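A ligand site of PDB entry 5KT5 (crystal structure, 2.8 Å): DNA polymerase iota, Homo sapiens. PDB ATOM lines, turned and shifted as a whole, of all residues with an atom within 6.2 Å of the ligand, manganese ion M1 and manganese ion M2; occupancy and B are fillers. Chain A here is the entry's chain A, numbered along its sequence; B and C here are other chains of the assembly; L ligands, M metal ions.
NZ of Lys 102 is in salt-bridge range of O2 of the ligand, 2.4 Å away. OG1 of Thr 90 is in hydrogen-bond range of O4 of the ligand, 2.6 Å away. O6 of DG 3 of chain C sits at hydrogen-bond distance from a nitrogen (N4) of the ligand. An oxygen (O3) of the ligand sits at hydrogen-bond distance from the backbone NH (N) of Cys 62, at 3.0 Å. The side-chain amino group (NZ) of Lys 239 is in salt-bridge range of an oxygen (O2) of the ligand (3.3 Å). O11 of the ligand lies within hydrogen-bond range of N of Tyr 64. O4 of the ligand is in hydrogen-bond range of N of Phe 63 (3.4 Å).
O2 of DC 7 of chain B sits close to N2 of DG 4 of chain C (2.7 Å). O4' of DG 4 of chain C lies within hydrogen-bond range of NE2 of Gln 84, at 3.4 Å.
An oxygen (O12) of the ligand sits close to N2 of DG 4 of chain C. Asp 61 touches the ligand (CA to O3, 3.5 Å). CG2 of Val 89 touches O12 of the ligand, at 3.2 Å. Leu 103 touches the ligand. Hydrophobic or aromatic side chains that line the ligand: Phe 63, Tyr 64, Val 89 and Leu 103. Within 4 Å of the ligand: Asp 59, Leu 60, Asp 61, Cys 62, Phe 63, Tyr 64, Val 89, Thr 90, Lys 102, Leu 103, Asp 151, Lys 239, DC 7 of chain B, DG 3 of chain C and DG 4 of chain C.
Four residues have an atom within 4 Å of manganese ion M1: Asp 59, Asp 151, Glu 152 and DC 7 of chain B.
The nearest printed residue that does not touch manganese ion M2 is Asp 61 (4.4 Å).
Manganese ion M1 is bound by O8 of the ligand (1.9 Å), O3' of DC 7 of chain B (2.2 Å), OE2 of Glu 152 (2.3 Å), OD1 of Asp 59 (2.3 Å) and OD1 of Asp 151 (2.5 Å). Slightly farther from manganese ion M1 lies OD2 of Asp 151 (2.9 Å).
Manganese ion M2 is bound by an oxygen (O5) of the ligand (1.9 Å), the side-chain carboxylate (OD2) of Asp 59 (2.0 Å), an oxygen (O1) of the ligand (2.1 Å), the side-chain carboxylate (OD2) of Asp 151 (2.1 Å), the backbone carbonyl oxygen (O) of Leu 60 (2.2 Å) and an oxygen (O8) of the ligand (2.4 Å). Manganese ion M2 has six donor atoms within binding distance.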
ATOM      1  N   ASP A  59      28.314 -26.513  -5.430  1.00  0.00           N
ATOM      2  CA  ASP A  59      27.148 -25.645  -5.484  1.00  0.00           C
ATOM      3  C   ASP A  59      27.103 -24.823  -4.195  1.00  0.00           C
ATOM      4  O   ASP A  59      27.142 -25.392  -3.102  1.00  0.00           O
ATOM      5  CB  ASP A  59      25.864 -26.472  -5.634  1.00  0.00           C
ATOM      6  CG  ASP A  59      24.601 -25.619  -5.735  1.00  0.00           C
ATOM      7  OD1 ASP A  59      23.818 -25.833  -6.678  1.00  0.00           O
ATOM      8  OD2 ASP A  59      24.370 -24.753  -4.872  1.00  0.00           O
ATOM      9  N   LEU A  60      27.001 -23.515  -4.320  1.00  0.00           N
ATOM     10  CA  LEU A  60      27.070 -22.636  -3.154  1.00  0.00           C
ATOM     11  C   LEU A  60      25.739 -22.624  -2.409  1.00  0.00           C
ATOM     12  O   LEU A  60      24.673 -22.632  -3.011  1.00  0.00           O
ATOM     13  CB  LEU A  60      27.440 -21.222  -3.580  1.00  0.00           C
ATOM     14  CG  LEU A  60      28.795 -21.155  -4.288  1.00  0.00           C
ATOM     15  CD1 LEU A  60      29.203 -19.726  -4.578  1.00  0.00           C
ATOM     16  CD2 LEU A  60      29.835 -21.841  -3.428  1.00  0.00           C
ATOM     17  N   ASP A  61      25.833 -22.609  -1.076  1.00  0.00           N
ATOM     18  CA  ASP A  61      24.646 -22.505  -0.233  1.00  0.00           C
ATOM     19  C   ASP A  61      24.016 -21.126  -0.367  1.00  0.00           C
ATOM     20  O   ASP A  61      24.700 -20.115  -0.194  1.00  0.00           O
ATOM     21  CB  ASP A  61      25.023 -22.763   1.223  1.00  0.00           C
ATOM     22  CG  ASP A  61      25.707 -24.115   1.437  1.00  0.00           C
ATOM     23  OD1 ASP A  61      25.178 -25.147   0.962  1.00  0.00           O
ATOM     24  OD2 ASP A  61      26.774 -24.137   2.080  1.00  0.00           O
ATOM     25  N   CYS A  62      22.704 -21.109  -0.653  1.00  0.00           N
ATOM     26  CA  CYS A  62      21.898 -19.903  -0.837  1.00  0.00           C
ATOM     27  C   CYS A  62      22.724 -18.718  -1.310  1.00  0.00           C
ATOM     28  O   CYS A  62      22.941 -17.757  -0.566  1.00  0.00           O
ATOM     29  CB  CYS A  62      21.156 -19.543   0.462  1.00  0.00           C
ATOM     30  SG  CYS A  62      22.185 -19.538   1.955  1.00  0.00           S
ATOM     31  N   PHE A  63      23.191 -18.787  -2.558  1.00  0.00           N
ATOM     32  CA  PHE A  63      24.325 -17.984  -2.990  1.00  0.00           C
ATOM     33  C   PHE A  63      24.103 -16.488  -2.745  1.00  0.00           C
ATOM     34  O   PHE A  63      24.808 -15.848  -1.955  1.00  0.00           O
ATOM     35  CB  PHE A  63      24.620 -18.283  -4.457  1.00  0.00           C
ATOM     36  CG  PHE A  63      25.760 -17.469  -5.024  1.00  0.00           C
ATOM     37  CD1 PHE A  63      26.911 -17.226  -4.294  1.00  0.00           C
ATOM     38  CD2 PHE A  63      25.666 -16.945  -6.312  1.00  0.00           C
ATOM     39  CE1 PHE A  63      27.945 -16.479  -4.824  1.00  0.00           C
ATOM     40  CE2 PHE A  63      26.690 -16.197  -6.839  1.00  0.00           C
ATOM     41  CZ  PHE A  63      27.834 -15.964  -6.097  1.00  0.00           C
ATOM     42  N   TYR A  64      23.107 -15.917  -3.433  1.00  0.00           N
ATOM     43  CA  TYR A  64      22.814 -14.496  -3.285  1.00  0.00           C
ATOM     44  C   TYR A  64      22.647 -14.102  -1.819  1.00  0.00           C
ATOM     45  O   TYR A  64      23.213 -13.101  -1.356  1.00  0.00           O
ATOM     46  CB  TYR A  64      21.545 -14.133  -4.071  1.00  0.00           C
ATOM     47  CG  TYR A  64      21.659 -14.244  -5.577  1.00  0.00           C
ATOM     48  CD1 TYR A  64      22.833 -14.671  -6.197  1.00  0.00           C
ATOM     49  CD2 TYR A  64      20.597 -13.888  -6.398  1.00  0.00           C
ATOM     50  CE1 TYR A  64      22.932 -14.764  -7.574  1.00  0.00           C
ATOM     51  CE2 TYR A  64      20.686 -13.980  -7.773  1.00  0.00           C
ATOM     52  CZ  TYR A  64      21.849 -14.418  -8.359  1.00  0.00           C
ATOM     53  OH  TYR A  64      21.928 -14.500  -9.730  1.00  0.00           O
ATOM     54  N   ALA A  65      21.869 -14.894  -1.069  1.00  0.00           N
ATOM     55  CA  ALA A  65      21.651 -14.577   0.335  1.00  0.00           C
ATOM     56  C   ALA A  65      22.954 -14.641   1.130  1.00  0.00           C
ATOM     57  O   ALA A  65      23.158 -13.874   2.080  1.00  0.00           O
ATOM     58  CB  ALA A  65      20.621 -15.526   0.942  1.00  0.00           C
ATOM     59  N   GLN A  84      13.791 -10.223  -6.432  1.00  0.00           N
ATOM     60  CA  GLN A  84      13.888  -9.595  -7.758  1.00  0.00           C
ATOM     61  C   GLN A  84      12.465  -9.450  -8.280  1.00  0.00           C
ATOM     62  O   GLN A  84      11.810 -10.450  -8.575  1.00  0.00           O
ATOM     63  CB  GLN A  84      14.738 -10.425  -8.716  1.00  0.00           C
ATOM     64  CG  GLN A  84      16.206 -10.519  -8.340  1.00  0.00           C
ATOM     65  CD  GLN A  84      16.963 -11.497  -9.204  1.00  0.00           C
ATOM     66  OE1 GLN A  84      16.401 -12.488  -9.689  1.00  0.00           O
ATOM     67  NE2 GLN A  84      18.243 -11.234  -9.410  1.00  0.00           N
ATOM     68  N   VAL A  89      14.024 -14.910  -4.889  1.00  0.00           N
ATOM     69  CA  VAL A  89      14.823 -15.800  -5.721  1.00  0.00           C
ATOM     70  C   VAL A  89      15.607 -16.805  -4.882  1.00  0.00           C
ATOM     71  O   VAL A  89      15.954 -17.893  -5.368  1.00  0.00           O
ATOM     72  CB  VAL A  89      15.742 -14.981  -6.643  1.00  0.00           C
ATOM     73  CG1 VAL A  89      17.101 -14.736  -5.990  1.00  0.00           C
ATOM     74  CG2 VAL A  89      15.905 -15.678  -7.970  1.00  0.00           C
ATOM     75  N   THR A  90      15.919 -16.457  -3.631  1.00  0.00           N
ATOM     76  CA  THR A  90      16.545 -17.388  -2.696  1.00  0.00           C
ATOM     77  C   THR A  90      16.467 -16.786  -1.311  1.00  0.00           C
ATOM     78  O   THR A  90      16.082 -15.622  -1.124  1.00  0.00           O
ATOM     79  CB  THR A  90      18.011 -17.691  -3.061  1.00  0.00           C
ATOM     80  OG1 THR A  90      18.504 -18.715  -2.185  1.00  0.00           O
ATOM     81  CG2 THR A  90      18.865 -16.446  -2.907  1.00  0.00           C
ATOM     82  N   CYS A  91      16.832 -17.597  -0.323  1.00  0.00           N
ATOM     83  CA  CYS A  91      16.697 -17.193   1.072  1.00  0.00           C
ATOM     84  C   CYS A  91      17.717 -17.947   1.905  1.00  0.00           C
ATOM     85  O   CYS A  91      18.176 -19.031   1.524  1.00  0.00           O
ATOM     86  CB  CYS A  91      15.274 -17.434   1.587  1.00  0.00           C
ATOM     87  SG  CYS A  91      14.772 -19.168   1.688  1.00  0.00           S
ATOM     88  N   LYS A 102      12.787 -21.247  -2.358  1.00  0.00           N
ATOM     89  CA  LYS A 102      13.386 -20.542  -3.487  1.00  0.00           C
ATOM     90  C   LYS A 102      12.365 -20.354  -4.594  1.00  0.00           C
ATOM     91  O   LYS A 102      11.549 -21.237  -4.883  1.00  0.00           O
ATOM     92  CB  LYS A 102      14.599 -21.323  -3.993  1.00  0.00           C
ATOM     93  CG  LYS A 102      15.715 -21.464  -2.962  1.00  0.00           C
ATOM     94  CD  LYS A 102      16.822 -22.392  -3.422  1.00  0.00           C
ATOM     95  CE  LYS A 102      16.411 -23.858  -3.329  1.00  0.00           C
ATOM     96  NZ  LYS A 102      17.564 -24.792  -3.543  1.00  0.00           N
ATOM     97  N   LEU A 103      12.410 -19.175  -5.228  1.00  0.00           N
ATOM     98  CA  LEU A 103      11.513 -18.821  -6.322  1.00  0.00           C
ATOM     99  C   LEU A 103      10.048 -18.770  -5.882  1.00  0.00           C
ATOM    100  O   LEU A 103       9.132 -19.051  -6.656  1.00  0.00           O
ATOM    101  CB  LEU A 103      11.683 -19.780  -7.513  1.00  0.00           C
ATOM    102  CG  LEU A 103      13.133 -19.931  -7.994  1.00  0.00           C
ATOM    103  CD1 LEU A 103      13.262 -21.051  -9.012  1.00  0.00           C
ATOM    104  CD2 LEU A 103      13.634 -18.630  -8.572  1.00  0.00           C
ATOM    105  N   LEU A 124      23.198  -7.986 -10.265  1.00  0.00           N
ATOM    106  CA  LEU A 124      23.996  -9.192 -10.068  1.00  0.00           C
ATOM    107  C   LEU A 124      25.501  -8.912 -10.024  1.00  0.00           C
ATOM    108  O   LEU A 124      26.284  -9.863 -10.147  1.00  0.00           O
ATOM    109  CB  LEU A 124      23.707 -10.194 -11.187  1.00  0.00           C
ATOM    110  CG  LEU A 124      22.256 -10.449 -11.609  1.00  0.00           C
ATOM    111  CD1 LEU A 124      22.214 -11.563 -12.643  1.00  0.00           C
ATOM    112  CD2 LEU A 124      21.377 -10.783 -10.415  1.00  0.00           C
ATOM    113  N   LEU A 148      28.603 -23.843 -14.269  1.00  0.00           N
ATOM    114  CA  LEU A 148      27.167 -23.963 -14.462  1.00  0.00           C
ATOM    115  C   LEU A 148      26.493 -22.929 -13.568  1.00  0.00           C
ATOM    116  O   LEU A 148      26.641 -22.985 -12.334  1.00  0.00           O
ATOM    117  CB  LEU A 148      26.651 -25.379 -14.153  1.00  0.00           C
ATOM    118  CG  LEU A 148      25.238 -25.665 -14.658  1.00  0.00           C
ATOM    119  CD1 LEU A 148      25.128 -25.327 -16.132  1.00  0.00           C
ATOM    120  CD2 LEU A 148      24.838 -27.114 -14.411  1.00  0.00           C
ATOM    121  N   PHE A 150      25.817 -19.185 -11.896  1.00  0.00           N
ATOM    122  CA  PHE A 150      26.766 -18.374 -11.147  1.00  0.00           C
ATOM    123  C   PHE A 150      27.380 -19.128  -9.976  1.00  0.00           C
ATOM    124  O   PHE A 150      28.425 -18.697  -9.471  1.00  0.00           O
ATOM    125  CB  PHE A 150      26.081 -17.114 -10.627  1.00  0.00           C
ATOM    126  CG  PHE A 150      25.965 -16.012 -11.655  1.00  0.00           C
ATOM    127  CD1 PHE A 150      25.562 -14.740 -11.283  1.00  0.00           C
ATOM    128  CD2 PHE A 150      26.258 -16.243 -12.984  1.00  0.00           C
ATOM    129  CE1 PHE A 150      25.459 -13.721 -12.213  1.00  0.00           C
ATOM    130  CE2 PHE A 150      26.162 -15.243 -13.927  1.00  0.00           C
ATOM    131  CZ  PHE A 150      25.761 -13.982 -13.546  1.00  0.00           C
ATOM    132  N   ASP A 151      26.787 -20.232  -9.533  1.00  0.00           N
ATOM    133  CA  ASP A 151      27.173 -20.828  -8.265  1.00  0.00           C
ATOM    134  C   ASP A 151      27.552 -22.303  -8.355  1.00  0.00           C
ATOM    135  O   ASP A 151      27.699 -22.946  -7.314  1.00  0.00           O
ATOM    136  CB  ASP A 151      26.061 -20.639  -7.233  1.00  0.00           C
ATOM    137  CG  ASP A 151      25.045 -21.770  -7.235  1.00  0.00           C
ATOM    138  OD1 ASP A 151      24.626 -22.206  -8.336  1.00  0.00           O
ATOM    139  OD2 ASP A 151      24.676 -22.243  -6.132  1.00  0.00           O
ATOM    140  N   GLU A 152      27.714 -22.871  -9.554  1.00  0.00           N
ATOM    141  CA  GLU A 152      28.093 -24.276  -9.653  1.00  0.00           C
ATOM    142  C   GLU A 152      29.321 -24.441 -10.530  1.00  0.00           C
ATOM    143  O   GLU A 152      29.488 -23.742 -11.531  1.00  0.00           O
ATOM    144  CB  GLU A 152      26.927 -25.122 -10.168  1.00  0.00           C
ATOM    145  CG  GLU A 152      25.787 -25.202  -9.166  1.00  0.00           C
ATOM    146  CD  GLU A 152      24.572 -25.896  -9.725  1.00  0.00           C
ATOM    147  OE1 GLU A 152      24.737 -26.800 -10.561  1.00  0.00           O
ATOM    148  OE2 GLU A 152      23.449 -25.537  -9.328  1.00  0.00           O
ATOM    149  N   LYS A 239      22.738 -31.163   2.730  1.00  0.00           N
ATOM    150  CA  LYS A 239      22.782 -29.712   2.663  1.00  0.00           C
ATOM    151  C   LYS A 239      22.403 -29.098   4.006  1.00  0.00           C
ATOM    152  O   LYS A 239      21.596 -29.678   4.738  1.00  0.00           O
ATOM    153  CB  LYS A 239      21.845 -29.197   1.553  1.00  0.00           C
ATOM    154  CG  LYS A 239      22.365 -29.416   0.141  1.00  0.00           C
ATOM    155  CD  LYS A 239      21.278 -29.206  -0.906  1.00  0.00           C
ATOM    156  CE  LYS A 239      20.497 -27.917  -0.670  1.00  0.00           C
ATOM    157  NZ  LYS A 239      19.454 -27.699  -1.708  1.00  0.00           N
ATOM    158  N   PRO A 240      22.980 -27.935   4.336  1.00  0.00           N
ATOM    159  CA  PRO A 240      23.995 -27.222   3.551  1.00  0.00           C
ATOM    160  C   PRO A 240      25.412 -27.487   4.029  1.00  0.00           C
ATOM    161  O   PRO A 240      25.594 -28.151   5.051  1.00  0.00           O
ATOM    162  CB  PRO A 240      23.623 -25.760   3.784  1.00  0.00           C
ATOM    163  CG  PRO A 240      23.160 -25.754   5.205  1.00  0.00           C
ATOM    164  CD  PRO A 240      22.485 -27.102   5.456  1.00  0.00           C
ATOM    165  P    DC B   7      19.879 -26.998 -12.989  1.00  0.00           P
ATOM    166  OP1  DC B   7      20.323 -28.091 -12.092  1.00  0.00           O
ATOM    167  OP2  DC B   7      18.456 -26.905 -13.388  1.00  0.00           O
ATOM    168  O5'  DC B   7      20.319 -25.604 -12.356  1.00  0.00           O
ATOM    169  C5'  DC B   7      21.692 -25.384 -12.028  1.00  0.00           C
ATOM    170  C4'  DC B   7      21.956 -23.918 -11.709  1.00  0.00           C
ATOM    171  O4'  DC B   7      21.727 -23.120 -12.880  1.00  0.00           O
ATOM    172  C3'  DC B   7      21.050 -23.298 -10.659  1.00  0.00           C
ATOM    173  O3'  DC B   7      21.509 -23.637  -9.351  1.00  0.00           O
ATOM    174  C2'  DC B   7      21.232 -21.819 -10.948  1.00  0.00           C
ATOM    175  C1'  DC B   7      21.375 -21.801 -12.480  1.00  0.00           C
ATOM    176  N1   DC B   7      20.130 -21.410 -13.178  1.00  0.00           N
ATOM    177  C2   DC B   7      19.787 -20.064 -13.246  1.00  0.00           C
ATOM    178  O2   DC B   7      20.546 -19.242 -12.736  1.00  0.00           O
ATOM    179  N3   DC B   7      18.632 -19.708 -13.876  1.00  0.00           N
ATOM    180  C4   DC B   7      17.853 -20.649 -14.405  1.00  0.00           C
ATOM    181  N4   DC B   7      16.736 -20.255 -15.014  1.00  0.00           N
ATOM    182  C5   DC B   7      18.183 -22.034 -14.345  1.00  0.00           C
ATOM    183  C6   DC B   7      19.326 -22.370 -13.721  1.00  0.00           C
ATOM    184  P    DG C   3       8.498 -11.280 -12.932  1.00  0.00           P
ATOM    185  OP1  DG C   3       7.556 -10.165 -12.729  1.00  0.00           O
ATOM    186  OP2  DG C   3       8.630 -11.895 -14.270  1.00  0.00           O
ATOM    187  O5'  DG C   3       9.969 -10.835 -12.501  1.00  0.00           O
ATOM    188  C5'  DG C   3      10.907 -11.830 -12.087  1.00  0.00           C
ATOM    189  C4'  DG C   3      12.235 -11.218 -11.706  1.00  0.00           C
ATOM    190  O4'  DG C   3      13.109 -12.252 -11.183  1.00  0.00           O
ATOM    191  C3'  DG C   3      13.016 -10.581 -12.845  1.00  0.00           C
ATOM    192  O3'  DG C   3      13.889  -9.593 -12.320  1.00  0.00           O
ATOM    193  C2'  DG C   3      13.788 -11.774 -13.397  1.00  0.00           C
ATOM    194  C1'  DG C   3      14.145 -12.520 -12.104  1.00  0.00           C
ATOM    195  N9   DG C   3      14.280 -13.974 -12.252  1.00  0.00           N
ATOM    196  C8   DG C   3      15.271 -14.753 -11.713  1.00  0.00           C
ATOM    197  N7   DG C   3      15.132 -16.024 -11.978  1.00  0.00           N
ATOM    198  C5   DG C   3      13.970 -16.096 -12.732  1.00  0.00           C
ATOM    199  C6   DG C   3      13.319 -17.212 -13.300  1.00  0.00           C
ATOM    200  O6   DG C   3      13.651 -18.407 -13.256  1.00  0.00           O
ATOM    201  N1   DG C   3      12.159 -16.845 -13.991  1.00  0.00           N
ATOM    202  C2   DG C   3      11.698 -15.553 -14.101  1.00  0.00           C
ATOM    203  N2   DG C   3      10.568 -15.397 -14.806  1.00  0.00           N
ATOM    204  N3   DG C   3      12.295 -14.495 -13.572  1.00  0.00           N
ATOM    205  C4   DG C   3      13.419 -14.840 -12.902  1.00  0.00           C
ATOM    206  P    DG C   4      14.484  -8.421 -13.259  1.00  0.00           P
ATOM    207  OP1  DG C   4      14.451  -7.161 -12.480  1.00  0.00           O
ATOM    208  OP2  DG C   4      13.813  -8.494 -14.571  1.00  0.00           O
ATOM    209  O5'  DG C   4      16.009  -8.849 -13.467  1.00  0.00           O
ATOM    210  C5'  DG C   4      16.826  -9.120 -12.338  1.00  0.00           C
ATOM    211  C4'  DG C   4      18.053  -9.913 -12.754  1.00  0.00           C
ATOM    212  O4'  DG C   4      17.707 -11.330 -12.812  1.00  0.00           O
ATOM    213  C3'  DG C   4      18.601  -9.563 -14.138  1.00  0.00           C
ATOM    214  O3'  DG C   4      20.033  -9.531 -14.101  1.00  0.00           O
ATOM    215  C2'  DG C   4      18.089 -10.710 -14.993  1.00  0.00           C
ATOM    216  C1'  DG C   4      18.203 -11.851 -14.007  1.00  0.00           C
ATOM    217  N9   DG C   4      17.467 -13.046 -14.420  1.00  0.00           N
ATOM    218  C8   DG C   4      16.287 -13.098 -15.127  1.00  0.00           C
ATOM    219  N7   DG C   4      15.886 -14.319 -15.372  1.00  0.00           N
ATOM    220  C5   DG C   4      16.857 -15.118 -14.786  1.00  0.00           C
ATOM    221  C6   DG C   4      16.968 -16.525 -14.729  1.00  0.00           C
ATOM    222  O6   DG C   4      16.191 -17.377 -15.183  1.00  0.00           O
ATOM    223  N1   DG C   4      18.115 -16.922 -14.046  1.00  0.00           N
ATOM    224  C2   DG C   4      19.042 -16.067 -13.497  1.00  0.00           C
ATOM    225  N2   DG C   4      20.091 -16.619 -12.885  1.00  0.00           N
ATOM    226  N3   DG C   4      18.950 -14.741 -13.551  1.00  0.00           N
ATOM    227  C4   DG C   4      17.840 -14.346 -14.213  1.00  0.00           C
HETATM  228  P1  LIG L   1      21.054 -23.799  -2.360  1.00  0.00           P
HETATM  229  O1  LIG L   1      22.118 -24.015  -3.411  1.00  0.00           O
HETATM  230  O2  LIG L   1      19.782 -24.575  -2.626  1.00  0.00           O
HETATM  231  O3  LIG L   1      21.561 -23.892  -0.945  1.00  0.00           O
HETATM  232  P2  LIG L   1      20.792 -21.442  -3.895  1.00  0.00           P
HETATM  233  O4  LIG L   1      20.251 -20.054  -3.628  1.00  0.00           O
HETATM  234  O5  LIG L   1      22.241 -21.544  -4.312  1.00  0.00           O
HETATM  235  O6  LIG L   1      20.619 -22.258  -2.522  1.00  0.00           O
HETATM  236  P3  LIG L   1      20.533 -22.339  -6.709  1.00  0.00           P
HETATM  237  O7  LIG L   1      19.530 -23.035  -7.596  1.00  0.00           O
HETATM  238  O8  LIG L   1      21.892 -22.986  -6.546  1.00  0.00           O
HETATM  239  N1  LIG L   1      19.766 -22.183  -5.129  1.00  0.00           N
HETATM  240  O9  LIG L   1      20.799 -20.898  -7.365  1.00  0.00           O
HETATM  241  C1  LIG L   1      22.004 -20.169  -7.113  1.00  0.00           C
HETATM  242  C2  LIG L   1      21.652 -18.692  -7.227  1.00  0.00           C
HETATM  243  O10 LIG L   1      21.228 -18.394  -8.555  1.00  0.00           O
HETATM  244  C3  LIG L   1      20.491 -18.339  -6.322  1.00  0.00           C
HETATM  245  O11 LIG L   1      20.933 -17.766  -5.079  1.00  0.00           O
HETATM  246  C4  LIG L   1      19.669 -17.333  -7.109  1.00  0.00           C
HETATM  247  C5  LIG L   1      20.108 -17.498  -8.559  1.00  0.00           C
HETATM  248  N2  LIG L   1      18.992 -18.072  -9.308  1.00  0.00           N
HETATM  249  C6  LIG L   1      18.098 -17.264 -10.028  1.00  0.00           C
HETATM  250  N3  LIG L   1      17.067 -17.823 -10.696  1.00  0.00           N
HETATM  251  C7  LIG L   1      16.887 -19.168 -10.683  1.00  0.00           C
HETATM  252  C8  LIG L   1      17.766 -19.974  -9.979  1.00  0.00           C
HETATM  253  C9  LIG L   1      18.825 -19.397  -9.287  1.00  0.00           C
HETATM  254  O12 LIG L   1      18.251 -16.019 -10.047  1.00  0.00           O
HETATM  255  N4  LIG L   1      15.853 -19.726 -11.360  1.00  0.00           N
HETATM  256 MN    MN M   1      22.958 -23.941  -7.721  1.00  0.00          MN
HETATM  257 MN    MN M   2      23.373 -23.024  -4.721  1.00  0.00          MN
